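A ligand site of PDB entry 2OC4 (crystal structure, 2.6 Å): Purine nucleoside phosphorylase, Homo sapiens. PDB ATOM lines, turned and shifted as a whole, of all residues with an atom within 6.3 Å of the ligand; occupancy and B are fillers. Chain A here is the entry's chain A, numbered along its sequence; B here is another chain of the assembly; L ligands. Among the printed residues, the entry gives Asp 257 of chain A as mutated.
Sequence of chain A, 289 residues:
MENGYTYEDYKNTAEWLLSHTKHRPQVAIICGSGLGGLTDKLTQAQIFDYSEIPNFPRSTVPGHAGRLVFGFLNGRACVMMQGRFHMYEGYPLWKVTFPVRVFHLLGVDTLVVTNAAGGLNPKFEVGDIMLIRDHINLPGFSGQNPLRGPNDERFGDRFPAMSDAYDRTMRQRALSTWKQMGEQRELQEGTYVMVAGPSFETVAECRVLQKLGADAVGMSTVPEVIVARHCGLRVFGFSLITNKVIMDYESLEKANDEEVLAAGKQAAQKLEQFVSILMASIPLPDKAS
The backbone carbonyl oxygen of Asn 243 is in hydrogen-bond range of the backbone NH of Gly 119, at 2.7 Å.
The backbone NH (N) of Met 219 sits at hydrogen-bond distance from the side-chain hydroxyl (OH) of Tyr 192 (3.1 Å).
The side-chain hydroxyl (OH) of Tyr 88 is in hydrogen-bond range of a ring nitrogen (ND1) of His 86, at 3.3 Å.
The backbone NH of Val 195 sits at hydrogen-bond distance from the backbone carbonyl oxygen of Gly 218 (3.1 Å).
OH of Tyr 192 sits close to O of Gly 218, at 3.3 Å.
N of Gly 118 lies within hydrogen-bond range of O of Val 217 (2.9 Å).
The backbone NH (N) of Thr 242 sits at hydrogen-bond distance from the backbone carbonyl oxygen (O) of Ala 117, 3.0 Å away.
The backbone carbonyl oxygen of Gly 119 is in hydrogen-bond range of the backbone NH of Val 245 (3.0 Å).
A nitrogen (N3) of the ligand lies within hydrogen-bond range of the side-chain carboxylate (OE1) of Glu 201 (2.8 Å).
An oxygen (O1) of the ligand lies within hydrogen-bond range of the side-chain carboxylate (OD1) of Asp 257 (2.9 Å).
OD1 of Asn 243 sits at hydrogen-bond distance from N2 of the ligand (3.0 Å).
The backbone NH (N) of Met 219 lies within hydrogen-bond range of an oxygen (O3) of the ligand (3.0 Å).
The side-chain hydroxyl (OH) of Tyr 88 is in hydrogen-bond range of an oxygen (O2) of the ligand, 3.4 Å away.
N of Gly 118 lies close to N2 of the ligand (3.5 Å).
His 86 touches the ligand.
Ala 116 touches the ligand.
C of Ala 117 touches N2 of the ligand, 3.7 Å away.
Phe 200 touches the ligand.
Val 217 touches the ligand (CG1 to N3, 3.5 Å).
Gly 218 touches the ligand.
Thr 242 touches the ligand.
Val 245 touches the ligand.
CG2 of Val 260 touches O1 of the ligand (3.6 Å).
Phe 159 of chain B touches the ligand (CE2 to C1, 3.5 Å).
Hydrophobic or aromatic side chains within 4 Å of the ligand: Tyr 88, Phe 200, Val 217, Met 219, Val 245, Val 260 and Phe 159 of chain B.
Within 4 Å of the ligand: His 86, Tyr 88, Ala 116, Ala 117, Gly 118, Phe 200, Glu 201, Val 217, Gly 218, Met 219, Thr 242, Asn 243, Val 245, Asp 257, Val 260 and Phe 159 of chain B.
Along chain A the residues within 4 Å of the ligand span positions 86 to 260.
The nearest printed residue that does not touch the ligand is Ser 220 (4.5 Å).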
ATOM      1  N   HIS A  86      11.135  18.913  -9.382  1.00  0.00           N
ATOM      2  CA  HIS A  86      10.133  17.938  -9.050  1.00  0.00           C
ATOM      3  C   HIS A  86       9.604  17.320 -10.321  1.00  0.00           C
ATOM      4  O   HIS A  86       9.553  17.977 -11.356  1.00  0.00           O
ATOM      5  CB  HIS A  86       8.936  18.550  -8.359  1.00  0.00           C
ATOM      6  CG  HIS A  86       9.266  19.332  -7.127  1.00  0.00           C
ATOM      7  ND1 HIS A  86       9.739  20.618  -7.169  1.00  0.00           N
ATOM      8  CD2 HIS A  86       9.112  19.037  -5.815  1.00  0.00           C
ATOM      9  CE1 HIS A  86       9.920  21.067  -5.944  1.00  0.00           C
ATOM     10  NE2 HIS A  86       9.518  20.132  -5.108  1.00  0.00           N
ATOM     11  N   TYR A  88       6.410  16.470 -10.740  1.00  0.00           N
ATOM     12  CA  TYR A  88       5.272  17.242 -11.159  1.00  0.00           C
ATOM     13  C   TYR A  88       5.566  18.448 -12.009  1.00  0.00           C
ATOM     14  O   TYR A  88       4.685  18.874 -12.695  1.00  0.00           O
ATOM     15  CB  TYR A  88       4.355  17.656 -10.006  1.00  0.00           C
ATOM     16  CG  TYR A  88       4.954  18.683  -9.069  1.00  0.00           C
ATOM     17  CD1 TYR A  88       4.973  20.042  -9.415  1.00  0.00           C
ATOM     18  CD2 TYR A  88       5.508  18.289  -7.842  1.00  0.00           C
ATOM     19  CE1 TYR A  88       5.560  20.967  -8.584  1.00  0.00           C
ATOM     20  CE2 TYR A  88       6.036  19.190  -7.003  1.00  0.00           C
ATOM     21  CZ  TYR A  88       6.065  20.532  -7.353  1.00  0.00           C
ATOM     22  OH  TYR A  88       6.659  21.424  -6.511  1.00  0.00           O
ATOM     23  N   ASN A 115      11.866  18.114   3.613  1.00  0.00           N
ATOM     24  CA  ASN A 115      10.745  18.438   2.759  1.00  0.00           C
ATOM     25  C   ASN A 115       9.576  18.796   3.604  1.00  0.00           C
ATOM     26  O   ASN A 115       9.636  18.654   4.792  1.00  0.00           O
ATOM     27  CB  ASN A 115      10.412  17.253   1.799  1.00  0.00           C
ATOM     28  CG  ASN A 115      10.018  15.969   2.525  1.00  0.00           C
ATOM     29  OD1 ASN A 115       9.214  15.982   3.447  1.00  0.00           O
ATOM     30  ND2 ASN A 115      10.574  14.846   2.085  1.00  0.00           N
ATOM     31  N   ALA A 116       8.507  19.275   2.988  1.00  0.00           N
ATOM     32  CA  ALA A 116       7.236  19.454   3.681  1.00  0.00           C
ATOM     33  C   ALA A 116       6.367  18.274   3.318  1.00  0.00           C
ATOM     34  O   ALA A 116       6.530  17.696   2.254  1.00  0.00           O
ATOM     35  CB  ALA A 116       6.597  20.740   3.213  1.00  0.00           C
ATOM     36  N   ALA A 117       5.411  17.888   4.149  1.00  0.00           N
ATOM     37  CA  ALA A 117       4.681  16.664   3.818  1.00  0.00           C
ATOM     38  C   ALA A 117       3.432  16.658   4.612  1.00  0.00           C
ATOM     39  O   ALA A 117       3.400  17.298   5.636  1.00  0.00           O
ATOM     40  CB  ALA A 117       5.533  15.430   4.135  1.00  0.00           C
ATOM     41  N   GLY A 118       2.406  15.977   4.130  1.00  0.00           N
ATOM     42  CA  GLY A 118       1.119  15.924   4.822  1.00  0.00           C
ATOM     43  C   GLY A 118       1.193  14.776   5.794  1.00  0.00           C
ATOM     44  O   GLY A 118       1.843  13.743   5.517  1.00  0.00           O
ATOM     45  N   GLY A 119       0.560  14.952   6.965  1.00  0.00           N
ATOM     46  CA  GLY A 119       0.611  13.916   7.957  1.00  0.00           C
ATOM     47  C   GLY A 119      -0.515  12.969   7.671  1.00  0.00           C
ATOM     48  O   GLY A 119      -1.638  13.398   7.404  1.00  0.00           O
ATOM     49  N   TYR A 192       7.915   7.678   4.828  1.00  0.00           N
ATOM     50  CA  TYR A 192       7.505   8.719   3.884  1.00  0.00           C
ATOM     51  C   TYR A 192       7.011   8.046   2.579  1.00  0.00           C
ATOM     52  O   TYR A 192       7.668   7.140   2.065  1.00  0.00           O
ATOM     53  CB  TYR A 192       8.699   9.591   3.508  1.00  0.00           C
ATOM     54  CG  TYR A 192       8.416  10.666   2.472  1.00  0.00           C
ATOM     55  CD1 TYR A 192       7.956  11.964   2.851  1.00  0.00           C
ATOM     56  CD2 TYR A 192       8.653  10.440   1.122  1.00  0.00           C
ATOM     57  CE1 TYR A 192       7.727  12.958   1.899  1.00  0.00           C
ATOM     58  CE2 TYR A 192       8.460  11.444   0.168  1.00  0.00           C
ATOM     59  CZ  TYR A 192       7.988  12.698   0.555  1.00  0.00           C
ATOM     60  OH  TYR A 192       7.785  13.682  -0.390  1.00  0.00           O
ATOM     61  N   VAL A 195       4.223  10.437  -3.756  1.00  0.00           N
ATOM     62  CA  VAL A 195       3.294  10.407  -4.852  1.00  0.00           C
ATOM     63  C   VAL A 195       3.731  11.543  -5.754  1.00  0.00           C
ATOM     64  O   VAL A 195       4.569  12.335  -5.367  1.00  0.00           O
ATOM     65  CB  VAL A 195       1.853  10.624  -4.403  1.00  0.00           C
ATOM     66  CG1 VAL A 195       1.438   9.573  -3.401  1.00  0.00           C
ATOM     67  CG2 VAL A 195       1.663  12.024  -3.880  1.00  0.00           C
ATOM     68  N   PRO A 198       0.826  17.074  -9.259  1.00  0.00           N
ATOM     69  CA  PRO A 198       0.901  18.181  -8.304  1.00  0.00           C
ATOM     70  C   PRO A 198      -0.371  18.471  -7.530  1.00  0.00           C
ATOM     71  O   PRO A 198      -0.348  19.355  -6.663  1.00  0.00           O
ATOM     72  CB  PRO A 198       1.117  19.361  -9.193  1.00  0.00           C
ATOM     73  CG  PRO A 198       0.264  19.035 -10.401  1.00  0.00           C
ATOM     74  CD  PRO A 198       0.456  17.553 -10.598  1.00  0.00           C
ATOM     75  N   SER A 199      -1.483  17.770  -7.821  1.00  0.00           N
ATOM     76  CA  SER A 199      -2.730  17.983  -7.110  1.00  0.00           C
ATOM     77  C   SER A 199      -2.718  17.189  -5.821  1.00  0.00           C
ATOM     78  O   SER A 199      -1.966  16.248  -5.710  1.00  0.00           O
ATOM     79  CB  SER A 199      -3.918  17.587  -7.979  1.00  0.00           C
ATOM     80  OG  SER A 199      -3.835  16.245  -8.403  1.00  0.00           O
ATOM     81  N   PHE A 200      -3.536  17.557  -4.838  1.00  0.00           N
ATOM     82  CA  PHE A 200      -3.446  16.964  -3.508  1.00  0.00           C
ATOM     83  C   PHE A 200      -4.383  15.765  -3.428  1.00  0.00           C
ATOM     84  O   PHE A 200      -5.266  15.599  -4.265  1.00  0.00           O
ATOM     85  CB  PHE A 200      -3.883  17.968  -2.425  1.00  0.00           C
ATOM     86  CG  PHE A 200      -2.894  19.018  -2.117  1.00  0.00           C
ATOM     87  CD1 PHE A 200      -1.707  18.710  -1.479  1.00  0.00           C
ATOM     88  CD2 PHE A 200      -3.189  20.373  -2.361  1.00  0.00           C
ATOM     89  CE1 PHE A 200      -0.774  19.681  -1.116  1.00  0.00           C
ATOM     90  CE2 PHE A 200      -2.250  21.408  -2.011  1.00  0.00           C
ATOM     91  CZ  PHE A 200      -1.031  21.019  -1.350  1.00  0.00           C
ATOM     92  N   GLU A 201      -4.270  14.969  -2.395  1.00  0.00           N
ATOM     93  CA  GLU A 201      -4.923  13.684  -2.354  1.00  0.00           C
ATOM     94  C   GLU A 201      -6.429  13.786  -2.092  1.00  0.00           C
ATOM     95  O   GLU A 201      -6.859  14.669  -1.407  1.00  0.00           O
ATOM     96  CB  GLU A 201      -4.289  12.867  -1.240  1.00  0.00           C
ATOM     97  CG  GLU A 201      -2.867  12.436  -1.512  1.00  0.00           C
ATOM     98  CD  GLU A 201      -1.853  13.572  -1.368  1.00  0.00           C
ATOM     99  OE1 GLU A 201      -1.982  14.339  -0.376  1.00  0.00           O
ATOM    100  OE2 GLU A 201      -0.927  13.692  -2.250  1.00  0.00           O
ATOM    101  N   VAL A 217       3.130  11.997   3.524  1.00  0.00           N
ATOM    102  CA  VAL A 217       3.097  11.985   2.040  1.00  0.00           C
ATOM    103  C   VAL A 217       3.628  13.300   1.432  1.00  0.00           C
ATOM    104  O   VAL A 217       3.243  14.394   1.866  1.00  0.00           O
ATOM    105  CB  VAL A 217       1.673  11.798   1.528  1.00  0.00           C
ATOM    106  CG1 VAL A 217       0.833  12.989   1.925  1.00  0.00           C
ATOM    107  CG2 VAL A 217       1.694  11.693   0.024  1.00  0.00           C
ATOM    108  N   GLY A 218       4.494  13.211   0.429  1.00  0.00           N
ATOM    109  CA  GLY A 218       4.917  14.402  -0.281  1.00  0.00           C
ATOM    110  C   GLY A 218       5.288  14.034  -1.698  1.00  0.00           C
ATOM    111  O   GLY A 218       5.113  12.866  -2.099  1.00  0.00           O
ATOM    112  N   MET A 219       5.842  15.012  -2.428  1.00  0.00           N
ATOM    113  CA  MET A 219       6.067  14.856  -3.859  1.00  0.00           C
ATOM    114  C   MET A 219       7.514  14.908  -4.279  1.00  0.00           C
ATOM    115  O   MET A 219       7.792  15.286  -5.430  1.00  0.00           O
ATOM    116  CB  MET A 219       5.252  15.883  -4.639  1.00  0.00           C
ATOM    117  CG  MET A 219       3.813  15.974  -4.095  1.00  0.00           C
ATOM    118  SD  MET A 219       2.643  17.208  -4.772  1.00  0.00           S
ATOM    119  CE  MET A 219       3.871  18.270  -5.390  1.00  0.00           C
ATOM    120  N   SER A 220       8.455  14.491  -3.425  1.00  0.00           N
ATOM    121  CA  SER A 220       9.869  14.589  -3.827  1.00  0.00           C
ATOM    122  C   SER A 220      10.793  13.660  -3.042  1.00  0.00           C
ATOM    123  O   SER A 220      10.354  12.715  -2.423  1.00  0.00           O
ATOM    124  CB  SER A 220      10.341  15.985  -3.510  1.00  0.00           C
ATOM    125  OG  SER A 220      10.306  16.172  -2.093  1.00  0.00           O
ATOM    126  N   THR A 242       3.435  19.752   7.428  1.00  0.00           N
ATOM    127  CA  THR A 242       2.872  21.062   7.374  1.00  0.00           C
ATOM    128  C   THR A 242       1.382  21.051   7.441  1.00  0.00           C
ATOM    129  O   THR A 242       0.779  22.106   7.471  1.00  0.00           O
ATOM    130  CB  THR A 242       3.210  21.670   6.087  1.00  0.00           C
ATOM    131  OG1 THR A 242       2.799  20.772   5.062  1.00  0.00           O
ATOM    132  CG2 THR A 242       4.714  21.894   5.999  1.00  0.00           C
ATOM    133  N   ASN A 243       0.757  19.877   7.429  1.00  0.00           N
ATOM    134  CA  ASN A 243      -0.716  19.790   7.296  1.00  0.00           C
ATOM    135  C   ASN A 243      -1.208  18.382   7.572  1.00  0.00           C
ATOM    136  O   ASN A 243      -0.480  17.419   7.344  1.00  0.00           O
ATOM    137  CB  ASN A 243      -1.201  20.278   5.930  1.00  0.00           C
ATOM    138  CG  ASN A 243      -0.559  19.533   4.747  1.00  0.00           C
ATOM    139  OD1 ASN A 243       0.422  19.979   4.140  1.00  0.00           O
ATOM    140  ND2 ASN A 243      -1.111  18.378   4.414  1.00  0.00           N
ATOM    141  N   VAL A 245      -3.628  15.481   6.695  1.00  0.00           N
ATOM    142  CA  VAL A 245      -4.263  15.160   5.449  1.00  0.00           C
ATOM    143  C   VAL A 245      -5.586  14.648   5.882  1.00  0.00           C
ATOM    144  O   VAL A 245      -5.726  14.248   7.015  1.00  0.00           O
ATOM    145  CB  VAL A 245      -3.486  14.062   4.787  1.00  0.00           C
ATOM    146  CG1 VAL A 245      -4.046  13.751   3.484  1.00  0.00           C
ATOM    147  CG2 VAL A 245      -2.093  14.481   4.646  1.00  0.00           C
ATOM    148  N   ALA A 255      -6.554  20.854   1.760  1.00  0.00           N
ATOM    149  CA  ALA A 255      -5.114  21.133   1.840  1.00  0.00           C
ATOM    150  C   ALA A 255      -4.737  22.200   0.826  1.00  0.00           C
ATOM    151  O   ALA A 255      -5.180  22.169  -0.316  1.00  0.00           O
ATOM    152  CB  ALA A 255      -4.322  19.862   1.635  1.00  0.00           C
ATOM    153  N   ASN A 256      -3.946  23.178   1.259  1.00  0.00           N
ATOM    154  CA  ASN A 256      -3.490  24.251   0.371  1.00  0.00           C
ATOM    155  C   ASN A 256      -2.015  24.515   0.558  1.00  0.00           C
ATOM    156  O   ASN A 256      -1.356  23.938   1.451  1.00  0.00           O
ATOM    157  CB  ASN A 256      -4.294  25.547   0.595  1.00  0.00           C
ATOM    158  CG  ASN A 256      -4.473  25.894   2.083  1.00  0.00           C
ATOM    159  OD1 ASN A 256      -3.580  26.459   2.736  1.00  0.00           O
ATOM    160  ND2 ASN A 256      -5.659  25.557   2.621  1.00  0.00           N
ATOM    161  N   ASP A 257      -1.485  25.389  -0.296  1.00  0.00           N
ATOM    162  CA  ASP A 257      -0.069  25.720  -0.251  1.00  0.00           C
ATOM    163  C   ASP A 257       0.222  27.003   0.580  1.00  0.00           C
ATOM    164  O   ASP A 257       1.392  27.294   0.912  1.00  0.00           O
ATOM    165  CB  ASP A 257       0.481  25.778  -1.686  1.00  0.00           C
ATOM    166  CG  ASP A 257       1.978  25.743  -1.737  1.00  0.00           C
ATOM    167  OD1 ASP A 257       2.589  24.758  -1.265  1.00  0.00           O
ATOM    168  OD2 ASP A 257       2.546  26.727  -2.249  1.00  0.00           O
ATOM    169  N   VAL A 260       1.298  25.421   3.887  1.00  0.00           N
ATOM    170  CA  VAL A 260       2.607  24.751   3.757  1.00  0.00           C
ATOM    171  C   VAL A 260       3.765  25.750   3.890  1.00  0.00           C
ATOM    172  O   VAL A 260       4.749  25.487   4.587  1.00  0.00           O
ATOM    173  CB  VAL A 260       2.719  23.969   2.410  1.00  0.00           C
ATOM    174  CG1 VAL A 260       4.124  23.344   2.226  1.00  0.00           C
ATOM    175  CG2 VAL A 260       1.610  22.913   2.296  1.00  0.00           C
ATOM    176  N   PHE B 159      -0.960  23.633  -7.011  1.00  0.00           N
ATOM    177  CA  PHE B 159      -1.320  22.505  -6.153  1.00  0.00           C
ATOM    178  C   PHE B 159      -2.837  22.513  -5.761  1.00  0.00           C
ATOM    179  O   PHE B 159      -3.198  22.717  -4.590  1.00  0.00           O
ATOM    180  CB  PHE B 159      -0.448  22.470  -4.861  1.00  0.00           C
ATOM    181  CG  PHE B 159       1.061  22.601  -5.103  1.00  0.00           C
ATOM    182  CD1 PHE B 159       1.805  21.535  -5.569  1.00  0.00           C
ATOM    183  CD2 PHE B 159       1.723  23.775  -4.829  1.00  0.00           C
ATOM    184  CE1 PHE B 159       3.229  21.652  -5.810  1.00  0.00           C
ATOM    185  CE2 PHE B 159       3.094  23.910  -5.026  1.00  0.00           C
ATOM    186  CZ  PHE B 159       3.866  22.836  -5.544  1.00  0.00           C
HETATM  187  O1  LIG L   1       2.202  21.915  -1.145  1.00  0.00           O
HETATM  188  C1  LIG L   1       3.192  21.872  -2.186  1.00  0.00           C
HETATM  189  C2  LIG L   1       4.487  21.251  -1.714  1.00  0.00           C
HETATM  190  N1  LIG L   1       4.513  20.642  -0.375  1.00  0.00           N
HETATM  191  C3  LIG L   1       4.814  20.107  -2.665  1.00  0.00           C
HETATM  192  O2  LIG L   1       6.070  20.444  -3.339  1.00  0.00           O
HETATM  193  C4  LIG L   1       4.787  18.812  -1.828  1.00  0.00           C
HETATM  194  O3  LIG L   1       5.925  17.982  -2.059  1.00  0.00           O
HETATM  195  C5  LIG L   1       4.693  19.168  -0.319  1.00  0.00           C
HETATM  196  C6  LIG L   1       3.477  18.659   0.386  1.00  0.00           C
HETATM  197  C7  LIG L   1       3.036  19.279   1.544  1.00  0.00           C
HETATM  198  N2  LIG L   1       1.871  18.634   1.926  1.00  0.00           N
HETATM  199  C8  LIG L   1       1.519  17.664   1.063  1.00  0.00           C
HETATM  200  C9  LIG L   1       0.422  16.714   0.924  1.00  0.00           C
HETATM  201  O4  LIG L   1      -0.528  16.709   1.863  1.00  0.00           O
HETATM  202  N3  LIG L   1       0.398  15.845  -0.119  1.00  0.00           N
HETATM  203  C10 LIG L   1       1.365  15.832  -1.035  1.00  0.00           C
HETATM  204  N4  LIG L   1       2.404  16.688  -0.995  1.00  0.00           N
HETATM  205  C11 LIG L   1       2.515  17.605   0.005  1.00  0.00           C
